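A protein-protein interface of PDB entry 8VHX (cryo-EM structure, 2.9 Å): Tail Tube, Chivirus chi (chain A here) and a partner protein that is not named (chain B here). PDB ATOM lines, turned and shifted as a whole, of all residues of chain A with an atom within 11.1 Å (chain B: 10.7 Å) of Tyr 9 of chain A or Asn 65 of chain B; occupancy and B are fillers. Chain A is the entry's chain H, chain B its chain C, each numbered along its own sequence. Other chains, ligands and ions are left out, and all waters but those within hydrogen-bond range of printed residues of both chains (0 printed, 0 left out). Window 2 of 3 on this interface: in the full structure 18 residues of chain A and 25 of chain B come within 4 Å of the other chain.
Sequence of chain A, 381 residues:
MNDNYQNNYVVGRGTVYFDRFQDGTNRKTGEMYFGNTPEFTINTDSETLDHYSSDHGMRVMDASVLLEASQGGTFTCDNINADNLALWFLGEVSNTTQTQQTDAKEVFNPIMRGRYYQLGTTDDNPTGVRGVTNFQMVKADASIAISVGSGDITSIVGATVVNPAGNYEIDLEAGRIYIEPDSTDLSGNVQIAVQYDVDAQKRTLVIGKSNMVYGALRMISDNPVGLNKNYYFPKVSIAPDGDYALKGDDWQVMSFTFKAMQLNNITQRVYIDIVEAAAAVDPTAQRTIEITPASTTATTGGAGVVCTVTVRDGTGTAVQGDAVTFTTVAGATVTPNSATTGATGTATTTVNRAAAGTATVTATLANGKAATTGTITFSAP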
ATOM      1  N   TYR A   5      -6.268  16.597  12.721  1.00  0.00           N
ATOM      2  CA  TYR A   5      -4.785  16.531  12.612  1.00  0.00           C
ATOM      3  C   TYR A   5      -4.200  17.869  12.171  1.00  0.00           C
ATOM      4  O   TYR A   5      -3.801  18.683  13.000  1.00  0.00           O
ATOM      5  CB  TYR A   5      -4.367  15.444  11.628  1.00  0.00           C
ATOM      6  CG  TYR A   5      -2.888  15.453  11.331  1.00  0.00           C
ATOM      7  CD1 TYR A   5      -1.952  15.563  12.353  1.00  0.00           C
ATOM      8  CD2 TYR A   5      -2.423  15.368  10.028  1.00  0.00           C
ATOM      9  CE1 TYR A   5      -0.604  15.577  12.080  1.00  0.00           C
ATOM     10  CE2 TYR A   5      -1.078  15.385   9.750  1.00  0.00           C
ATOM     11  CZ  TYR A   5      -0.173  15.487  10.776  1.00  0.00           C
ATOM     12  OH  TYR A   5       1.168  15.501  10.486  1.00  0.00           O
ATOM     13  N   GLN A   6      -4.152  18.088  10.860  1.00  0.00           N
ATOM     14  CA  GLN A   6      -3.607  19.328  10.336  1.00  0.00           C
ATOM     15  C   GLN A   6      -4.345  20.518  10.931  1.00  0.00           C
ATOM     16  O   GLN A   6      -5.493  20.421  11.367  1.00  0.00           O
ATOM     17  CB  GLN A   6      -3.720  19.371   8.813  1.00  0.00           C
ATOM     18  CG  GLN A   6      -3.019  18.256   8.095  1.00  0.00           C
ATOM     19  CD  GLN A   6      -3.913  17.053   7.877  1.00  0.00           C
ATOM     20  OE1 GLN A   6      -4.930  16.892   8.550  1.00  0.00           O
ATOM     21  NE2 GLN A   6      -3.517  16.181   6.962  1.00  0.00           N
ATOM     22  N   ASN A   7      -3.658  21.650  10.965  1.00  0.00           N
ATOM     23  CA  ASN A   7      -4.305  22.895  11.337  1.00  0.00           C
ATOM     24  C   ASN A   7      -5.147  23.402  10.179  1.00  0.00           C
ATOM     25  O   ASN A   7      -4.672  23.507   9.048  1.00  0.00           O
ATOM     26  CB  ASN A   7      -3.271  23.935  11.743  1.00  0.00           C
ATOM     27  CG  ASN A   7      -2.676  23.671  13.103  1.00  0.00           C
ATOM     28  OD1 ASN A   7      -3.047  22.723  13.790  1.00  0.00           O
ATOM     29  ND2 ASN A   7      -1.778  24.546  13.524  1.00  0.00           N
ATOM     30  N   ASN A   8      -6.410  23.702  10.464  1.00  0.00           N
ATOM     31  CA  ASN A   8      -7.376  24.060   9.431  1.00  0.00           C
ATOM     32  C   ASN A   8      -7.418  25.574   9.294  1.00  0.00           C
ATOM     33  O   ASN A   8      -8.263  26.262   9.860  1.00  0.00           O
ATOM     34  CB  ASN A   8      -8.747  23.495   9.755  1.00  0.00           C
ATOM     35  CG  ASN A   8      -9.716  23.668   8.636  1.00  0.00           C
ATOM     36  OD1 ASN A   8      -9.415  23.377   7.484  1.00  0.00           O
ATOM     37  ND2 ASN A   8     -10.900  24.135   8.968  1.00  0.00           N
ATOM     38  N   TYR A   9      -6.471  26.091   8.530  1.00  0.00           N
ATOM     39  CA  TYR A   9      -6.508  27.486   8.138  1.00  0.00           C
ATOM     40  C   TYR A   9      -7.511  27.652   7.011  1.00  0.00           C
ATOM     41  O   TYR A   9      -7.463  26.929   6.014  1.00  0.00           O
ATOM     42  CB  TYR A   9      -5.123  27.943   7.715  1.00  0.00           C
ATOM     43  CG  TYR A   9      -4.042  27.626   8.708  1.00  0.00           C
ATOM     44  CD1 TYR A   9      -4.109  28.095   9.996  1.00  0.00           C
ATOM     45  CD2 TYR A   9      -2.947  26.868   8.354  1.00  0.00           C
ATOM     46  CE1 TYR A   9      -3.138  27.816  10.896  1.00  0.00           C
ATOM     47  CE2 TYR A   9      -1.969  26.590   9.259  1.00  0.00           C
ATOM     48  CZ  TYR A   9      -2.067  27.066  10.526  1.00  0.00           C
ATOM     49  OH  TYR A   9      -1.083  26.787  11.434  1.00  0.00           O
ATOM     50  N   VAL A  10      -8.426  28.600   7.171  1.00  0.00           N
ATOM     51  CA  VAL A  10      -9.656  28.646   6.398  1.00  0.00           C
ATOM     52  C   VAL A  10      -9.836  30.016   5.769  1.00  0.00           C
ATOM     53  O   VAL A  10      -9.563  31.043   6.397  1.00  0.00           O
ATOM     54  CB  VAL A  10     -10.866  28.304   7.281  1.00  0.00           C
ATOM     55  CG1 VAL A  10     -12.130  28.570   6.580  1.00  0.00           C
ATOM     56  CG2 VAL A  10     -10.821  26.894   7.662  1.00  0.00           C
ATOM     57  N   VAL A  11     -10.302  30.025   4.525  1.00  0.00           N
ATOM     58  CA  VAL A  11     -10.794  31.217   3.853  1.00  0.00           C
ATOM     59  C   VAL A  11     -12.281  31.022   3.610  1.00  0.00           C
ATOM     60  O   VAL A  11     -12.694  30.024   3.011  1.00  0.00           O
ATOM     61  CB  VAL A  11     -10.047  31.481   2.544  1.00  0.00           C
ATOM     62  CG1 VAL A  11     -10.743  32.521   1.764  1.00  0.00           C
ATOM     63  CG2 VAL A  11      -8.667  31.931   2.823  1.00  0.00           C
ATOM     64  N   GLY A  12     -13.086  31.971   4.076  1.00  0.00           N
ATOM     65  CA  GLY A  12     -14.518  31.759   4.149  1.00  0.00           C
ATOM     66  C   GLY A  12     -15.270  32.107   2.888  1.00  0.00           C
ATOM     67  O   GLY A  12     -15.072  33.173   2.298  1.00  0.00           O
ATOM     68  N   ARG A  13     -16.153  31.202   2.484  1.00  0.00           N
ATOM     69  CA  ARG A  13     -17.140  31.431   1.446  1.00  0.00           C
ATOM     70  C   ARG A  13     -18.337  30.550   1.762  1.00  0.00           C
ATOM     71  O   ARG A  13     -18.202  29.540   2.451  1.00  0.00           O
ATOM     72  CB  ARG A  13     -16.603  31.096   0.062  1.00  0.00           C
ATOM     73  CG  ARG A  13     -15.443  31.912  -0.393  1.00  0.00           C
ATOM     74  CD  ARG A  13     -15.803  33.333  -0.646  1.00  0.00           C
ATOM     75  NE  ARG A  13     -14.664  34.039  -1.217  1.00  0.00           N
ATOM     76  CZ  ARG A  13     -13.699  34.601  -0.504  1.00  0.00           C
ATOM     77  NH1 ARG A  13     -12.700  35.201  -1.117  1.00  0.00           N
ATOM     78  NH2 ARG A  13     -13.741  34.576   0.816  1.00  0.00           N
ATOM     79  N   SER A 221     -20.844  25.918   3.794  1.00  0.00           N
ATOM     80  CA  SER A 221     -19.471  26.380   3.603  1.00  0.00           C
ATOM     81  C   SER A 221     -18.919  26.059   2.224  1.00  0.00           C
ATOM     82  O   SER A 221     -18.873  24.896   1.827  1.00  0.00           O
ATOM     83  CB  SER A 221     -18.558  25.778   4.671  1.00  0.00           C
ATOM     84  OG  SER A 221     -18.055  26.777   5.538  1.00  0.00           O
ATOM     85  N   ASP A 222     -18.497  27.088   1.496  1.00  0.00           N
ATOM     86  CA  ASP A 222     -17.891  26.876   0.187  1.00  0.00           C
ATOM     87  C   ASP A 222     -16.427  27.260   0.273  1.00  0.00           C
ATOM     88  O   ASP A 222     -15.768  27.455  -0.748  1.00  0.00           O
ATOM     89  CB  ASP A 222     -18.599  27.704  -0.880  1.00  0.00           C
ATOM     90  CG  ASP A 222     -18.295  27.225  -2.285  1.00  0.00           C
ATOM     91  OD1 ASP A 222     -18.764  26.127  -2.655  1.00  0.00           O
ATOM     92  OD2 ASP A 222     -17.587  27.944  -3.021  1.00  0.00           O
ATOM     93  N   ASN A 223     -15.917  27.375   1.494  1.00  0.00           N
ATOM     94  CA  ASN A 223     -14.521  27.755   1.696  1.00  0.00           C
ATOM     95  C   ASN A 223     -13.596  27.160   0.646  1.00  0.00           C
ATOM     96  O   ASN A 223     -13.450  25.941   0.564  1.00  0.00           O
ATOM     97  CB  ASN A 223     -14.061  27.324   3.090  1.00  0.00           C
ATOM     98  CG  ASN A 223     -15.188  27.336   4.103  1.00  0.00           C
ATOM     99  OD1 ASN A 223     -16.023  28.242   4.109  1.00  0.00           O
ATOM    100  ND2 ASN A 223     -15.219  26.327   4.963  1.00  0.00           N
ATOM    101  N   PRO A 224     -12.959  28.021  -0.160  1.00  0.00           N
ATOM    102  CA  PRO A 224     -12.007  27.534  -1.161  1.00  0.00           C
ATOM    103  C   PRO A 224     -10.756  27.005  -0.484  1.00  0.00           C
ATOM    104  O   PRO A 224     -10.028  26.213  -1.081  1.00  0.00           O
ATOM    105  CB  PRO A 224     -11.680  28.791  -1.967  1.00  0.00           C
ATOM    106  CG  PRO A 224     -11.916  29.917  -1.020  1.00  0.00           C
ATOM    107  CD  PRO A 224     -13.063  29.490  -0.152  1.00  0.00           C
ATOM    108  N   VAL A 225     -10.506  27.437   0.747  1.00  0.00           N
ATOM    109  CA  VAL A 225      -9.348  26.964   1.492  1.00  0.00           C
ATOM    110  C   VAL A 225      -9.789  26.520   2.877  1.00  0.00           C
ATOM    111  O   VAL A 225     -10.424  27.286   3.602  1.00  0.00           O
ATOM    112  CB  VAL A 225      -8.276  28.058   1.624  1.00  0.00           C
ATOM    113  CG1 VAL A 225      -7.298  27.719   2.738  1.00  0.00           C
ATOM    114  CG2 VAL A 225      -7.545  28.246   0.303  1.00  0.00           C
ATOM    115  N   GLY A 226      -9.469  25.284   3.247  1.00  0.00           N
ATOM    116  CA  GLY A 226      -9.892  24.789   4.532  1.00  0.00           C
ATOM    117  C   GLY A 226     -11.154  23.959   4.457  1.00  0.00           C
ATOM    118  O   GLY A 226     -11.909  23.984   3.486  1.00  0.00           O
ATOM    119  N   LEU A 227     -11.373  23.202   5.521  1.00  0.00           N
ATOM    120  CA  LEU A 227     -12.530  22.341   5.592  1.00  0.00           C
ATOM    121  C   LEU A 227     -13.804  23.164   5.670  1.00  0.00           C
ATOM    122  O   LEU A 227     -13.808  24.322   6.091  1.00  0.00           O
ATOM    123  CB  LEU A 227     -12.450  21.427   6.804  1.00  0.00           C
ATOM    124  CG  LEU A 227     -11.219  20.565   6.969  1.00  0.00           C
ATOM    125  CD1 LEU A 227     -11.422  19.697   8.157  1.00  0.00           C
ATOM    126  CD2 LEU A 227     -10.969  19.736   5.765  1.00  0.00           C
ATOM    127  N   ASN A 228     -14.898  22.536   5.277  1.00  0.00           N
ATOM    128  CA  ASN A 228     -16.184  23.197   5.218  1.00  0.00           C
ATOM    129  C   ASN A 228     -16.991  22.882   6.463  1.00  0.00           C
ATOM    130  O   ASN A 228     -17.007  21.747   6.943  1.00  0.00           O
ATOM    131  CB  ASN A 228     -16.931  22.773   3.962  1.00  0.00           C
ATOM    132  CG  ASN A 228     -16.326  23.348   2.721  1.00  0.00           C
ATOM    133  OD1 ASN A 228     -16.164  24.555   2.601  1.00  0.00           O
ATOM    134  ND2 ASN A 228     -15.962  22.489   1.795  1.00  0.00           N
ATOM    135  N   LYS A 229     -17.651  23.903   6.990  1.00  0.00           N
ATOM    136  CA  LYS A 229     -18.464  23.784   8.186  1.00  0.00           C
ATOM    137  C   LYS A 229     -19.759  24.525   7.949  1.00  0.00           C
ATOM    138  O   LYS A 229     -19.745  25.690   7.545  1.00  0.00           O
ATOM    139  CB  LYS A 229     -17.752  24.353   9.403  1.00  0.00           C
ATOM    140  CG  LYS A 229     -16.610  23.528   9.860  1.00  0.00           C
ATOM    141  CD  LYS A 229     -15.838  24.226  10.902  1.00  0.00           C
ATOM    142  CE  LYS A 229     -14.914  23.291  11.573  1.00  0.00           C
ATOM    143  NZ  LYS A 229     -14.101  22.619  10.568  1.00  0.00           N
ATOM    144  N   GLY B  61       2.867  37.138   0.563  1.00  0.00           N
ATOM    145  CA  GLY B  61       1.539  36.647   0.833  1.00  0.00           C
ATOM    146  C   GLY B  61       1.054  36.958   2.229  1.00  0.00           C
ATOM    147  O   GLY B  61       1.783  37.430   3.097  1.00  0.00           O
ATOM    148  N   SER B  62      -0.232  36.696   2.430  1.00  0.00           N
ATOM    149  CA  SER B  62      -0.863  36.817   3.735  1.00  0.00           C
ATOM    150  C   SER B  62      -0.696  35.508   4.486  1.00  0.00           C
ATOM    151  O   SER B  62      -1.226  34.476   4.074  1.00  0.00           O
ATOM    152  CB  SER B  62      -2.333  37.165   3.582  1.00  0.00           C
ATOM    153  OG  SER B  62      -2.963  37.268   4.842  1.00  0.00           O
ATOM    154  N   PHE B  63       0.036  35.555   5.589  1.00  0.00           N
ATOM    155  CA  PHE B  63       0.389  34.352   6.314  1.00  0.00           C
ATOM    156  C   PHE B  63      -0.696  33.971   7.302  1.00  0.00           C
ATOM    157  O   PHE B  63      -1.289  34.824   7.964  1.00  0.00           O
ATOM    158  CB  PHE B  63       1.715  34.558   7.026  1.00  0.00           C
ATOM    159  CG  PHE B  63       2.851  34.807   6.097  1.00  0.00           C
ATOM    160  CD1 PHE B  63       3.531  33.762   5.531  1.00  0.00           C
ATOM    161  CD2 PHE B  63       3.220  36.087   5.762  1.00  0.00           C
ATOM    162  CE1 PHE B  63       4.553  33.985   4.676  1.00  0.00           C
ATOM    163  CE2 PHE B  63       4.250  36.302   4.900  1.00  0.00           C
ATOM    164  CZ  PHE B  63       4.913  35.254   4.359  1.00  0.00           C
ATOM    165  N   ALA B  64      -0.951  32.671   7.394  1.00  0.00           N
ATOM    166  CA  ALA B  64      -1.969  32.148   8.285  1.00  0.00           C
ATOM    167  C   ALA B  64      -1.459  31.938   9.688  1.00  0.00           C
ATOM    168  O   ALA B  64      -2.263  31.842  10.620  1.00  0.00           O
ATOM    169  CB  ALA B  64      -2.476  30.822   7.762  1.00  0.00           C
ATOM    170  N   ASN B  65      -0.149  31.860   9.851  1.00  0.00           N
ATOM    171  CA  ASN B  65       0.471  31.519  11.112  1.00  0.00           C
ATOM    172  C   ASN B  65       1.695  32.387  11.329  1.00  0.00           C
ATOM    173  O   ASN B  65       2.268  32.927  10.383  1.00  0.00           O
ATOM    174  CB  ASN B  65       0.886  30.058  11.118  1.00  0.00           C
ATOM    175  CG  ASN B  65       1.740  29.705   9.947  1.00  0.00           C
ATOM    176  OD1 ASN B  65       2.310  30.571   9.298  1.00  0.00           O
ATOM    177  ND2 ASN B  65       1.845  28.430   9.669  1.00  0.00           N
ATOM    178  N   GLU B  66       2.084  32.524  12.589  1.00  0.00           N
ATOM    179  CA  GLU B  66       3.476  32.790  12.864  1.00  0.00           C
ATOM    180  C   GLU B  66       4.280  31.615  12.340  1.00  0.00           C
ATOM    181  O   GLU B  66       3.722  30.633  11.875  1.00  0.00           O
ATOM    182  CB  GLU B  66       3.701  33.043  14.349  1.00  0.00           C
ATOM    183  CG  GLU B  66       3.433  31.892  15.290  1.00  0.00           C
ATOM    184  CD  GLU B  66       2.087  32.015  15.970  1.00  0.00           C
ATOM    185  OE1 GLU B  66       1.140  32.498  15.320  1.00  0.00           O
ATOM    186  OE2 GLU B  66       1.984  31.643  17.159  1.00  0.00           O
ATOM    187  N   GLU B  67       5.598  31.784  12.303  1.00  0.00           N
ATOM    188  CA  GLU B  67       6.531  30.883  11.625  1.00  0.00           C
ATOM    189  C   GLU B  67       6.321  30.965  10.116  1.00  0.00           C
ATOM    190  O   GLU B  67       7.034  30.311   9.353  1.00  0.00           O
ATOM    191  CB  GLU B  67       6.450  29.427  12.134  1.00  0.00           C
ATOM    192  CG  GLU B  67       5.268  28.559  11.736  1.00  0.00           C
ATOM    193  CD  GLU B  67       5.401  27.121  12.166  1.00  0.00           C
ATOM    194  OE1 GLU B  67       6.390  26.787  12.850  1.00  0.00           O
ATOM    195  OE2 GLU B  67       4.511  26.317  11.817  1.00  0.00           O
ATOM    196  N   GLN B  68       5.351  31.770   9.684  1.00  0.00           N
ATOM    197  CA  GLN B  68       5.252  32.253   8.310  1.00  0.00           C
ATOM    198  C   GLN B  68       5.463  31.145   7.292  1.00  0.00           C
ATOM    199  O   GLN B  68       6.257  31.263   6.359  1.00  0.00           O
ATOM    200  CB  GLN B  68       6.222  33.401   8.081  1.00  0.00           C
ATOM    201  CG  GLN B  68       5.823  34.642   8.823  1.00  0.00           C
ATOM    202  CD  GLN B  68       6.493  35.875   8.321  1.00  0.00           C
ATOM    203  OE1 GLN B  68       7.678  35.875   8.004  1.00  0.00           O
ATOM    204  NE2 GLN B  68       5.726  36.944   8.224  1.00  0.00           N
ATOM    205  N   THR B  69       4.720  30.063   7.466  1.00  0.00           N
ATOM    206  CA  THR B  69       4.862  28.876   6.643  1.00  0.00           C
ATOM    207  C   THR B  69       3.710  28.671   5.672  1.00  0.00           C
ATOM    208  O   THR B  69       3.931  28.167   4.570  1.00  0.00           O
ATOM    209  CB  THR B  69       4.984  27.651   7.544  1.00  0.00           C
ATOM    210  OG1 THR B  69       6.052  27.847   8.468  1.00  0.00           O
ATOM    211  CG2 THR B  69       5.305  26.477   6.753  1.00  0.00           C
ATOM    212  N   VAL B  70       2.493  29.033   6.057  1.00  0.00           N
ATOM    213  CA  VAL B  70       1.311  28.916   5.217  1.00  0.00           C
ATOM    214  C   VAL B  70       0.846  30.315   4.854  1.00  0.00           C
ATOM    215  O   VAL B  70       0.799  31.201   5.715  1.00  0.00           O
ATOM    216  CB  VAL B  70       0.195  28.140   5.929  1.00  0.00           C
ATOM    217  CG1 VAL B  70      -0.993  28.038   5.070  1.00  0.00           C
ATOM    218  CG2 VAL B  70       0.651  26.778   6.288  1.00  0.00           C
ATOM    219  N   ARG B  71       0.491  30.516   3.587  1.00  0.00           N
ATOM    220  CA  ARG B  71       0.095  31.833   3.124  1.00  0.00           C
ATOM    221  C   ARG B  71      -0.886  31.714   1.973  1.00  0.00           C
ATOM    222  O   ARG B  71      -0.950  30.697   1.283  1.00  0.00           O
ATOM    223  CB  ARG B  71       1.305  32.652   2.691  1.00  0.00           C
ATOM    224  CG  ARG B  71       1.925  32.163   1.440  1.00  0.00           C
ATOM    225  CD  ARG B  71       3.259  32.760   1.223  1.00  0.00           C
ATOM    226  NE  ARG B  71       3.683  32.581  -0.157  1.00  0.00           N
ATOM    227  CZ  ARG B  71       4.854  32.079  -0.529  1.00  0.00           C
ATOM    228  NH1 ARG B  71       5.136  31.948  -1.806  1.00  0.00           N
ATOM    229  NH2 ARG B  71       5.751  31.707   0.362  1.00  0.00           N
ATOM    230  N   MET B  72      -1.665  32.776   1.796  1.00  0.00           N
ATOM    231  CA  MET B  72      -2.473  32.998   0.604  1.00  0.00           C
ATOM    232  C   MET B  72      -1.705  33.882  -0.366  1.00  0.00           C
ATOM    233  O   MET B  72      -1.466  35.059  -0.089  1.00  0.00           O
ATOM    234  CB  MET B  72      -3.805  33.641   0.968  1.00  0.00           C
ATOM    235  CG  MET B  72      -4.694  33.960  -0.209  1.00  0.00           C
ATOM    236  SD  MET B  72      -5.256  32.561  -1.174  1.00  0.00           S
ATOM    237  CE  MET B  72      -5.958  31.591   0.124  1.00  0.00           C
ATOM    238  N   ALA B 130      -7.842  28.950  -4.979  1.00  0.00           N
ATOM    239  CA  ALA B 130      -8.936  29.501  -4.207  1.00  0.00           C
ATOM    240  C   ALA B 130      -9.695  30.583  -4.955  1.00  0.00           C
ATOM    241  O   ALA B 130     -10.913  30.704  -4.801  1.00  0.00           O
ATOM    242  CB  ALA B 130      -8.395  30.058  -2.902  1.00  0.00           C
ATOM    243  N   LEU B 160      -4.122  31.104  -4.130  1.00  0.00           N
ATOM    244  CA  LEU B 160      -3.790  29.730  -3.811  1.00  0.00           C
ATOM    245  C   LEU B 160      -3.127  29.682  -2.449  1.00  0.00           C
ATOM    246  O   LEU B 160      -2.384  30.588  -2.070  1.00  0.00           O
ATOM    247  CB  LEU B 160      -2.884  29.104  -4.874  1.00  0.00           C
ATOM    248  CG  LEU B 160      -1.450  29.587  -4.983  1.00  0.00           C
ATOM    249  CD1 LEU B 160      -0.603  28.573  -5.657  1.00  0.00           C
ATOM    250  CD2 LEU B 160      -1.427  30.814  -5.790  1.00  0.00           C
ATOM    251  N   LYS B 161      -3.423  28.621  -1.714  1.00  0.00           N
ATOM    252  CA  LYS B 161      -2.780  28.368  -0.437  1.00  0.00           C
ATOM    253  C   LYS B 161      -1.429  27.725  -0.677  1.00  0.00           C
ATOM    254  O   LYS B 161      -1.329  26.708  -1.370  1.00  0.00           O
ATOM    255  CB  LYS B 161      -3.652  27.476   0.430  1.00  0.00           C
ATOM    256  CG  LYS B 161      -3.066  27.142   1.758  1.00  0.00           C
ATOM    257  CD  LYS B 161      -3.734  25.951   2.359  1.00  0.00           C
ATOM    258  CE  LYS B 161      -3.166  25.650   3.706  1.00  0.00           C
ATOM    259  NZ  LYS B 161      -3.940  24.610   4.429  1.00  0.00           N
ATOM    260  N   VAL B 162      -0.392  28.317  -0.105  1.00  0.00           N
ATOM    261  CA  VAL B 162       0.965  27.822  -0.223  1.00  0.00           C
ATOM    262  C   VAL B 162       1.448  27.444   1.162  1.00  0.00           C
ATOM    263  O   VAL B 162       1.459  28.282   2.068  1.00  0.00           O
ATOM    264  CB  VAL B 162       1.890  28.873  -0.848  1.00  0.00           C
ATOM    265  CG1 VAL B 162       3.255  28.304  -1.072  1.00  0.00           C
ATOM    266  CG2 VAL B 162       1.312  29.376  -2.124  1.00  0.00           C
ATOM    267  N   ASP B 163       1.833  26.188   1.330  1.00  0.00           N
ATOM    268  CA  ASP B 163       2.586  25.739   2.486  1.00  0.00           C
ATOM    269  C   ASP B 163       3.976  25.384   1.993  1.00  0.00           C
ATOM    270  O   ASP B 163       4.145  24.409   1.256  1.00  0.00           O
ATOM    271  CB  ASP B 163       1.908  24.546   3.153  1.00  0.00           C
ATOM    272  CG  ASP B 163       2.580  24.135   4.443  1.00  0.00           C
ATOM    273  OD1 ASP B 163       3.772  24.449   4.625  1.00  0.00           O
ATOM    274  OD2 ASP B 163       1.914  23.494   5.280  1.00  0.00           O
ATOM    275  N   ILE B 164       4.967  26.183   2.392  1.00  0.00           N
ATOM    276  CA  ILE B 164       6.314  26.021   1.866  1.00  0.00           C
ATOM    277  C   ILE B 164       6.965  24.731   2.322  1.00  0.00           C
ATOM    278  O   ILE B 164       8.051  24.391   1.847  1.00  0.00           O
ATOM    279  CB  ILE B 164       7.177  27.233   2.254  1.00  0.00           C
ATOM    280  CG1 ILE B 164       7.390  27.283   3.757  1.00  0.00           C
ATOM    281  CG2 ILE B 164       6.531  28.504   1.791  1.00  0.00           C
ATOM    282  CD1 ILE B 164       8.196  28.443   4.183  1.00  0.00           C
ATOM    283  N   ARG B 165       6.331  24.008   3.236  1.00  0.00           N
ATOM    284  CA  ARG B 165       6.755  22.660   3.561  1.00  0.00           C
ATOM    285  C   ARG B 165       6.419  21.669   2.462  1.00  0.00           C
ATOM    286  O   ARG B 165       7.054  20.615   2.376  1.00  0.00           O
ATOM    287  CB  ARG B 165       6.095  22.216   4.856  1.00  0.00           C
ATOM    288  CG  ARG B 165       6.482  23.024   6.057  1.00  0.00           C
ATOM    289  CD  ARG B 165       5.611  22.679   7.234  1.00  0.00           C
ATOM    290  NE  ARG B 165       4.261  23.202   7.077  1.00  0.00           N
ATOM    291  CZ  ARG B 165       3.353  23.194   8.043  1.00  0.00           C
ATOM    292  NH1 ARG B 165       2.151  23.698   7.835  1.00  0.00           N
ATOM    293  NH2 ARG B 165       3.645  22.660   9.214  1.00  0.00           N
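Printed residues of chain B that touch a printed residue of chain A: Ala 64, Asn 65, Val 70, Met 72, Ala 130 and Lys 161. Hydrophobic or aromatic side chains of chain B within 4 Å of the printed part of chain A: Ala 64, Val 70, Met 72 and Ala 130. Of the 18 printed residues of chain A, 4 touch a printed residue of chain B. Along chain A the printed residues that touch a printed residue of chain B span positions 9 to 225.
CG of Tyr 9 of chain A touches CB of Ala 64 of chain B (3.7 Å). OH of Tyr 9 of chain A touches ND2 of Asn 65 of chain B (3.8 Å). Val 70 of chain B touches Tyr 9 of chain A (CG2 to CE2, 3.97 Å). Val 11 of chain A touches Met 72 of chain B (CG2 to CE, 3.8 Å). Ala 130 of chain B touches Pro 224 of chain A (O to CB, 3.5 Å). Met 72 of chain B touches Val 225 of chain A. Ala 130 of chain B touches Val 225 of chain A. Val 225 of chain A touches Lys 161 of chain B (CG2 to CB, 3.97 Å).
The backbone NH (N) of Ala 64 of chain B lies within hydrogen-bond range of the backbone carbonyl oxygen (O) of Val 70 of chain B, 2.8 Å away. OD1 of Asn 65 of chain B lies within hydrogen-bond range of N of Gln 68 of chain B (3.3 Å). The backbone NH (N) of Thr 69 of chain B is in hydrogen-bond range of the side-chain amide oxygen (OD1) of Asn 65 of chain B (3.1 Å). SD of Met 72 of chain B sits at hydrogen-bond distance from N of Leu 160 of chain B (3.5 Å). The side-chain amide nitrogen (ND2) of Asn 7 of chain A sits at hydrogen-bond distance from the side-chain hydroxyl (OH) of Tyr 9 of chain A (3.1 Å). The backbone NH (N) of Val 11 of chain A is in hydrogen-bond range of the backbone carbonyl oxygen (O) of Val 225 of chain A.
No residue of chain B comes within 4 Å of Asn 7 of chain A. Tyr 9 of chain A touches three residues of chain B. Printed residues of chain B within 4 Å of Pro 224 of chain A: Ala 130 (3.5 Å). Val 225 of chain A touches three residues of chain B. No residue of chain B comes within 4 Å of Gly 226 of chain A. No residue of chain A comes within 4 Å of Phe 63 of chain B. Ala 64 of chain B touches just one residue of chain A: Tyr 9 (3.7 Å). Printed residues of chain A within 4 Å of Asn 65 of chain B: Tyr 9. No residue of chain A comes within 4 Å of Glu 67 of chain B. Gln 68 of chain B touches none of the printed residues of chain A. Of the printed residues of chain A, Val 70 of chain B touches Tyr 9. Of the printed residues of chain A, Met 72 of chain B touches Val 11 and Val 225. Of the printed residues of chain A, Ala 130 of chain B touches Pro 224 and Val 225. The nearest residue of chain B that does not touch Tyr 9 of chain A is Lys 161 of chain B (4.5 Å).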
